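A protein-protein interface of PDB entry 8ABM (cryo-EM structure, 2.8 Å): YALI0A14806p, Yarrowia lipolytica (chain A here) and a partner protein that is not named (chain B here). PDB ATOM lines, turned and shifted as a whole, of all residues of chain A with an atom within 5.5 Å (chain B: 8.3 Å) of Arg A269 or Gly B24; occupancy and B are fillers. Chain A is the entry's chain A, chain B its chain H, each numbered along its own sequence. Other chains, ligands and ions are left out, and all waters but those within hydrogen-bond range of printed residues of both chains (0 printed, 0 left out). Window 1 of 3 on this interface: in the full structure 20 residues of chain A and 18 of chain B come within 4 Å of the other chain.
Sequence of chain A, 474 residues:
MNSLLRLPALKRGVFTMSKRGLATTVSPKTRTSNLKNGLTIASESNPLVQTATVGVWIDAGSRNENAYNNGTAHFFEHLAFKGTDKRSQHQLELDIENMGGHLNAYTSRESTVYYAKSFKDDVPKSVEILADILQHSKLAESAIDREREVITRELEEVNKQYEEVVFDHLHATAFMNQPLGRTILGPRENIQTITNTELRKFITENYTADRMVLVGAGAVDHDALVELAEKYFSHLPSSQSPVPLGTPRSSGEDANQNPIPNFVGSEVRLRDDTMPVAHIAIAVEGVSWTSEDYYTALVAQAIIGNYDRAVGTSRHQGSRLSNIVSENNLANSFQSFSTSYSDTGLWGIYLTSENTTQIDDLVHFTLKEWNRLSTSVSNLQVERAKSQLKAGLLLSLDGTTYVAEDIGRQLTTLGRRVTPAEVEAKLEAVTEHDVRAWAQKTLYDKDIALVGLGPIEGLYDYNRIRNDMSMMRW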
ATOM      1  N   GLU A 267      -3.820 -27.154 -10.378  1.00  0.00           N
ATOM      2  CA  GLU A 267      -2.497 -26.574 -10.459  1.00  0.00           C
ATOM      3  C   GLU A 267      -2.571 -25.275 -11.238  1.00  0.00           C
ATOM      4  O   GLU A 267      -3.378 -25.150 -12.149  1.00  0.00           O
ATOM      5  CB  GLU A 267      -1.552 -27.616 -11.037  1.00  0.00           C
ATOM      6  CG  GLU A 267      -0.717 -27.162 -12.188  1.00  0.00           C
ATOM      7  CD  GLU A 267      -0.438 -28.328 -13.121  1.00  0.00           C
ATOM      8  OE1 GLU A 267      -0.078 -29.429 -12.632  1.00  0.00           O
ATOM      9  OE2 GLU A 267      -0.605 -28.142 -14.337  1.00  0.00           O
ATOM     10  N   VAL A 268      -1.761 -24.312 -10.811  1.00  0.00           N
ATOM     11  CA  VAL A 268      -1.553 -23.084 -11.542  1.00  0.00           C
ATOM     12  C   VAL A 268      -0.073 -23.022 -11.870  1.00  0.00           C
ATOM     13  O   VAL A 268       0.741 -23.080 -10.952  1.00  0.00           O
ATOM     14  CB  VAL A 268      -1.916 -21.879 -10.670  1.00  0.00           C
ATOM     15  CG1 VAL A 268      -1.796 -20.602 -11.471  1.00  0.00           C
ATOM     16  CG2 VAL A 268      -3.299 -22.021 -10.076  1.00  0.00           C
ATOM     17  N   ARG A 269       0.260 -22.873 -13.152  1.00  0.00           N
ATOM     18  CA  ARG A 269       1.645 -22.615 -13.487  1.00  0.00           C
ATOM     19  C   ARG A 269       1.804 -21.205 -14.020  1.00  0.00           C
ATOM     20  O   ARG A 269       1.109 -20.804 -14.949  1.00  0.00           O
ATOM     21  CB  ARG A 269       2.095 -23.561 -14.587  1.00  0.00           C
ATOM     22  CG  ARG A 269       2.047 -25.005 -14.164  1.00  0.00           C
ATOM     23  CD  ARG A 269       2.366 -25.775 -15.420  1.00  0.00           C
ATOM     24  NE  ARG A 269       2.119 -27.093 -14.891  1.00  0.00           N
ATOM     25  CZ  ARG A 269       3.036 -27.947 -14.457  1.00  0.00           C
ATOM     26  NH1 ARG A 269       4.324 -27.655 -14.522  1.00  0.00           N
ATOM     27  NH2 ARG A 269       2.627 -29.095 -13.951  1.00  0.00           N
ATOM     28  N   LEU A 270       2.745 -20.471 -13.434  1.00  0.00           N
ATOM     29  CA  LEU A 270       2.994 -19.106 -13.843  1.00  0.00           C
ATOM     30  C   LEU A 270       4.445 -19.076 -14.273  1.00  0.00           C
ATOM     31  O   LEU A 270       5.320 -18.604 -13.552  1.00  0.00           O
ATOM     32  CB  LEU A 270       2.754 -18.196 -12.641  1.00  0.00           C
ATOM     33  CG  LEU A 270       1.393 -18.359 -11.969  1.00  0.00           C
ATOM     34  CD1 LEU A 270       1.426 -17.795 -10.556  1.00  0.00           C
ATOM     35  CD2 LEU A 270       0.315 -17.659 -12.781  1.00  0.00           C
ATOM     36  N   ARG A 271       4.691 -19.689 -15.418  1.00  0.00           N
ATOM     37  CA  ARG A 271       6.061 -19.815 -15.854  1.00  0.00           C
ATOM     38  C   ARG A 271       6.613 -18.443 -16.240  1.00  0.00           C
ATOM     39  O   ARG A 271       5.927 -17.654 -16.879  1.00  0.00           O
ATOM     40  CB  ARG A 271       6.113 -20.808 -17.003  1.00  0.00           C
ATOM     41  CG  ARG A 271       7.473 -20.864 -17.670  1.00  0.00           C
ATOM     42  CD  ARG A 271       7.526 -22.234 -18.286  1.00  0.00           C
ATOM     43  NE  ARG A 271       8.666 -22.196 -19.177  1.00  0.00           N
ATOM     44  CZ  ARG A 271       8.912 -23.077 -20.131  1.00  0.00           C
ATOM     45  NH1 ARG A 271       8.094 -24.099 -20.333  1.00  0.00           N
ATOM     46  NH2 ARG A 271       9.989 -22.926 -20.881  1.00  0.00           N
ATOM     47  N   LEU A 450      -1.262 -27.206  -6.447  1.00  0.00           N
ATOM     48  CA  LEU A 450       0.138 -27.036  -6.758  1.00  0.00           C
ATOM     49  C   LEU A 450       0.286 -25.711  -7.486  1.00  0.00           C
ATOM     50  O   LEU A 450      -0.461 -25.429  -8.414  1.00  0.00           O
ATOM     51  CB  LEU A 450       0.518 -28.223  -7.636  1.00  0.00           C
ATOM     52  CG  LEU A 450       1.759 -28.021  -8.491  1.00  0.00           C
ATOM     53  CD1 LEU A 450       3.019 -28.159  -7.667  1.00  0.00           C
ATOM     54  CD2 LEU A 450       1.774 -29.070  -9.574  1.00  0.00           C
ATOM     55  N   GLY A 452       3.246 -23.174  -9.248  1.00  0.00           N
ATOM     56  CA  GLY A 452       4.637 -22.982  -9.574  1.00  0.00           C
ATOM     57  C   GLY A 452       4.803 -21.625 -10.227  1.00  0.00           C
ATOM     58  O   GLY A 452       3.987 -21.232 -11.056  1.00  0.00           O
ATOM     59  N   ILE A 456       9.929 -22.987 -14.366  1.00  0.00           N
ATOM     60  CA  ILE A 456       9.392 -24.226 -13.835  1.00  0.00           C
ATOM     61  C   ILE A 456       9.147 -25.193 -14.989  1.00  0.00           C
ATOM     62  O   ILE A 456       8.329 -26.104 -14.881  1.00  0.00           O
ATOM     63  CB  ILE A 456       8.092 -23.931 -13.061  1.00  0.00           C
ATOM     64  CG1 ILE A 456       7.132 -23.141 -13.958  1.00  0.00           C
ATOM     65  CG2 ILE A 456       8.378 -23.206 -11.756  1.00  0.00           C
ATOM     66  CD1 ILE A 456       5.695 -23.079 -13.502  1.00  0.00           C
ATOM     67  N   LEU A 459       9.229 -28.703 -13.948  1.00  0.00           N
ATOM     68  CA  LEU A 459       8.241 -29.268 -13.050  1.00  0.00           C
ATOM     69  C   LEU A 459       7.312 -30.097 -13.925  1.00  0.00           C
ATOM     70  O   LEU A 459       6.809 -29.568 -14.910  1.00  0.00           O
ATOM     71  CB  LEU A 459       7.532 -28.089 -12.383  1.00  0.00           C
ATOM     72  CG  LEU A 459       6.379 -28.450 -11.455  1.00  0.00           C
ATOM     73  CD1 LEU A 459       6.879 -29.214 -10.247  1.00  0.00           C
ATOM     74  CD2 LEU A 459       5.620 -27.212 -11.014  1.00  0.00           C
ATOM     75  N   TYR A 460       7.148 -31.392 -13.623  1.00  0.00           N
ATOM     76  CA  TYR A 460       6.315 -32.234 -14.472  1.00  0.00           C
ATOM     77  C   TYR A 460       4.853 -31.837 -14.345  1.00  0.00           C
ATOM     78  O   TYR A 460       4.502 -31.087 -13.447  1.00  0.00           O
ATOM     79  CB  TYR A 460       6.460 -33.711 -14.116  1.00  0.00           C
ATOM     80  CG  TYR A 460       7.823 -34.253 -14.445  1.00  0.00           C
ATOM     81  CD1 TYR A 460       8.480 -33.865 -15.607  1.00  0.00           C
ATOM     82  CD2 TYR A 460       8.468 -35.131 -13.585  1.00  0.00           C
ATOM     83  CE1 TYR A 460       9.746 -34.341 -15.906  1.00  0.00           C
ATOM     84  CE2 TYR A 460       9.726 -35.635 -13.882  1.00  0.00           C
ATOM     85  CZ  TYR A 460      10.366 -35.231 -15.045  1.00  0.00           C
ATOM     86  OH  TYR A 460      11.610 -35.703 -15.347  1.00  0.00           O
ATOM     87  N   ASP A 461       4.020 -32.385 -15.225  1.00  0.00           N
ATOM     88  CA  ASP A 461       2.583 -32.164 -15.235  1.00  0.00           C
ATOM     89  C   ASP A 461       1.922 -32.684 -13.953  1.00  0.00           C
ATOM     90  O   ASP A 461       2.518 -33.423 -13.162  1.00  0.00           O
ATOM     91  CB  ASP A 461       2.004 -32.856 -16.466  1.00  0.00           C
ATOM     92  CG  ASP A 461       2.613 -34.238 -16.634  1.00  0.00           C
ATOM     93  OD1 ASP A 461       2.422 -35.057 -15.724  1.00  0.00           O
ATOM     94  OD2 ASP A 461       3.312 -34.474 -17.657  1.00  0.00           O
ATOM     95  N   TYR A 462       0.651 -32.317 -13.781  1.00  0.00           N
ATOM     96  CA  TYR A 462      -0.076 -32.663 -12.575  1.00  0.00           C
ATOM     97  C   TYR A 462       0.001 -34.152 -12.257  1.00  0.00           C
ATOM     98  O   TYR A 462       0.247 -34.484 -11.106  1.00  0.00           O
ATOM     99  CB  TYR A 462      -1.531 -32.213 -12.646  1.00  0.00           C
ATOM    100  CG  TYR A 462      -2.235 -32.338 -11.326  1.00  0.00           C
ATOM    101  CD1 TYR A 462      -2.223 -31.291 -10.411  1.00  0.00           C
ATOM    102  CD2 TYR A 462      -2.908 -33.506 -10.984  1.00  0.00           C
ATOM    103  CE1 TYR A 462      -2.876 -31.410  -9.188  1.00  0.00           C
ATOM    104  CE2 TYR A 462      -3.562 -33.633  -9.765  1.00  0.00           C
ATOM    105  CZ  TYR A 462      -3.548 -32.581  -8.859  1.00  0.00           C
ATOM    106  OH  TYR A 462      -4.192 -32.716  -7.655  1.00  0.00           O
ATOM    107  N   ILE A 465       3.215 -35.386 -10.647  1.00  0.00           N
ATOM    108  CA  ILE A 465       3.393 -34.913  -9.287  1.00  0.00           C
ATOM    109  C   ILE A 465       2.444 -35.698  -8.389  1.00  0.00           C
ATOM    110  O   ILE A 465       2.853 -36.254  -7.386  1.00  0.00           O
ATOM    111  CB  ILE A 465       3.179 -33.392  -9.139  1.00  0.00           C
ATOM    112  CG1 ILE A 465       4.030 -32.499 -10.052  1.00  0.00           C
ATOM    113  CG2 ILE A 465       3.318 -32.978  -7.689  1.00  0.00           C
ATOM    114  CD1 ILE A 465       5.397 -33.009 -10.412  1.00  0.00           C
ATOM    115  N   TRP B  11      14.223 -31.607 -19.813  1.00  0.00           N
ATOM    116  CA  TRP B  11      13.441 -30.834 -18.876  1.00  0.00           C
ATOM    117  C   TRP B  11      14.321 -29.797 -18.199  1.00  0.00           C
ATOM    118  O   TRP B  11      15.381 -30.129 -17.675  1.00  0.00           O
ATOM    119  CB  TRP B  11      12.858 -31.784 -17.854  1.00  0.00           C
ATOM    120  CG  TRP B  11      12.006 -32.820 -18.503  1.00  0.00           C
ATOM    121  CD1 TRP B  11      12.335 -34.120 -18.752  1.00  0.00           C
ATOM    122  CD2 TRP B  11      10.671 -32.631 -18.996  1.00  0.00           C
ATOM    123  NE1 TRP B  11      11.281 -34.763 -19.339  1.00  0.00           N
ATOM    124  CE2 TRP B  11      10.250 -33.878 -19.511  1.00  0.00           C
ATOM    125  CE3 TRP B  11       9.796 -31.536 -19.054  1.00  0.00           C
ATOM    126  CZ2 TRP B  11       8.986 -34.055 -20.082  1.00  0.00           C
ATOM    127  CZ3 TRP B  11       8.547 -31.712 -19.617  1.00  0.00           C
ATOM    128  CH2 TRP B  11       8.153 -32.954 -20.123  1.00  0.00           C
ATOM    129  N   GLY B  21       4.200 -14.547 -19.012  1.00  0.00           N
ATOM    130  CA  GLY B  21       2.898 -13.951 -19.237  1.00  0.00           C
ATOM    131  C   GLY B  21       1.795 -14.980 -19.471  1.00  0.00           C
ATOM    132  O   GLY B  21       0.630 -14.603 -19.513  1.00  0.00           O
ATOM    133  N   ILE B  22       2.131 -16.270 -19.532  1.00  0.00           N
ATOM    134  CA  ILE B  22       1.077 -17.259 -19.664  1.00  0.00           C
ATOM    135  C   ILE B  22       0.808 -17.922 -18.319  1.00  0.00           C
ATOM    136  O   ILE B  22       1.718 -18.483 -17.722  1.00  0.00           O
ATOM    137  CB  ILE B  22       1.449 -18.305 -20.720  1.00  0.00           C
ATOM    138  CG1 ILE B  22       1.882 -17.653 -22.033  1.00  0.00           C
ATOM    139  CG2 ILE B  22       0.288 -19.270 -20.905  1.00  0.00           C
ATOM    140  CD1 ILE B  22       2.623 -18.592 -22.965  1.00  0.00           C
ATOM    141  N   ALA B  23      -0.450 -17.890 -17.868  1.00  0.00           N
ATOM    142  CA  ALA B  23      -0.849 -18.631 -16.685  1.00  0.00           C
ATOM    143  C   ALA B  23      -1.614 -19.856 -17.159  1.00  0.00           C
ATOM    144  O   ALA B  23      -2.534 -19.714 -17.958  1.00  0.00           O
ATOM    145  CB  ALA B  23      -1.705 -17.764 -15.800  1.00  0.00           C
ATOM    146  N   GLY B  24      -1.216 -21.042 -16.702  1.00  0.00           N
ATOM    147  CA  GLY B  24      -1.916 -22.255 -17.091  1.00  0.00           C
ATOM    148  C   GLY B  24      -2.659 -22.831 -15.894  1.00  0.00           C
ATOM    149  O   GLY B  24      -2.132 -22.807 -14.791  1.00  0.00           O
ATOM    150  N   TYR B  25      -3.880 -23.318 -16.102  1.00  0.00           N
ATOM    151  CA  TYR B  25      -4.639 -23.843 -14.993  1.00  0.00           C
ATOM    152  C   TYR B  25      -5.213 -25.184 -15.366  1.00  0.00           C
ATOM    153  O   TYR B  25      -5.701 -25.351 -16.475  1.00  0.00           O
ATOM    154  CB  TYR B  25      -5.875 -22.988 -14.780  1.00  0.00           C
ATOM    155  CG  TYR B  25      -5.508 -21.579 -14.456  1.00  0.00           C
ATOM    156  CD1 TYR B  25      -5.156 -20.698 -15.464  1.00  0.00           C
ATOM    157  CD2 TYR B  25      -5.477 -21.130 -13.144  1.00  0.00           C
ATOM    158  CE1 TYR B  25      -4.820 -19.386 -15.186  1.00  0.00           C
ATOM    159  CE2 TYR B  25      -5.124 -19.826 -12.845  1.00  0.00           C
ATOM    160  CZ  TYR B  25      -4.803 -18.954 -13.871  1.00  0.00           C
ATOM    161  OH  TYR B  25      -4.464 -17.669 -13.594  1.00  0.00           O
ATOM    162  N   THR B  26      -5.183 -26.132 -14.435  1.00  0.00           N
ATOM    163  CA  THR B  26      -5.874 -27.376 -14.706  1.00  0.00           C
ATOM    164  C   THR B  26      -6.371 -28.004 -13.417  1.00  0.00           C
ATOM    165  O   THR B  26      -5.971 -27.606 -12.339  1.00  0.00           O
ATOM    166  CB  THR B  26      -4.993 -28.334 -15.506  1.00  0.00           C
ATOM    167  OG1 THR B  26      -5.904 -29.350 -15.925  1.00  0.00           O
ATOM    168  CG2 THR B  26      -3.840 -28.903 -14.710  1.00  0.00           C
ATOM    169  N   ILE B  27      -7.217 -29.016 -13.538  1.00  0.00           N
ATOM    170  CA  ILE B  27      -7.735 -29.662 -12.347  1.00  0.00           C
ATOM    171  C   ILE B  27      -7.332 -31.133 -12.326  1.00  0.00           C
ATOM    172  O   ILE B  27      -7.008 -31.713 -13.361  1.00  0.00           O
ATOM    173  CB  ILE B  27      -9.252 -29.462 -12.261  1.00  0.00           C
ATOM    174  CG1 ILE B  27      -9.939 -30.053 -13.492  1.00  0.00           C
ATOM    175  CG2 ILE B  27      -9.569 -27.984 -12.072  1.00  0.00           C
ATOM    176  CD1 ILE B  27     -11.425 -30.217 -13.331  1.00  0.00           C
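The backbone carbonyl oxygen (O) of Leu A459 sits at hydrogen-bond distance from the guanidinium group (NH1) of Arg A269, at 3.2 Å.
The backbone NH of Tyr A462 lies close to the side-chain carboxylate of Glu A267 (3.2 Å).
The side-chain carboxylate (OE2) of Glu A267 is in salt-bridge range of the guanidinium group (NE) of Arg A269.
NH2 of Arg A269 sits at hydrogen-bond distance from O of Tyr A460, 2.8 Å away.
N of Gly A452 lies within hydrogen-bond range of O of Val A268 (3.0 Å).
The backbone NH (N) of Val A268 sits at hydrogen-bond distance from the backbone carbonyl oxygen (O) of Leu A450, 2.9 Å away.
Of the 13 printed residues of chain A, 6 touch a printed residue of chain B.
Hydrophobic or aromatic side chains of chain A that line the printed part of chain B: Val A268, Leu A270 and Tyr A460.
Of the printed residues of chain B, Arg A269 touches Ile B22, Ala B23 and Gly B24.
Of chain A, only Glu A267, Val A268 and Arg A269 come within 4 Å of Gly B24.
Printed residues of chain A within 4 Å of Trp B11: Tyr A460 (3.7 Å).
Of the printed residues of chain B, Leu A270 touches Ala B23 (3.6 Å).
Of the printed residues of chain B, Arg A271 touches Ile B22 (3.9 Å).
Of the printed residues of chain B, Tyr A460 touches Trp B11.
Printed residues of chain A within 4 Å of Tyr B25: Glu A267 (3.4 Å) and Val A268 (3.7 Å).
Leu A450 touches none of the printed residues of chain B.
Ile A465 touches none of the printed residues of chain B.
The backbone NH (N) of Arg A269 lies within hydrogen-bond range of the backbone carbonyl oxygen (O) of Gly B24 (2.9 Å).
The backbone NH of Glu A267 sits at hydrogen-bond distance from the backbone carbonyl oxygen of Thr B26, at 2.9 Å.
Among the printed residues, merely in contact across the chains: Val A268 with Gly B24 (3.3 Å), Glu A267 with Tyr B25 (3.4 Å), Arg A269 with Ala B23 (3.4 Å), Leu A270 with Ala B23 (3.6 Å), Tyr A460 with Trp B11 (3.7 Å), Arg A269 with Ile B22 (3.7 Å), Val A268 with Tyr B25 (3.7 Å), Glu A267 with Gly B24 (3.7 Å) and Arg A271 with Ile B22 (3.9 Å).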
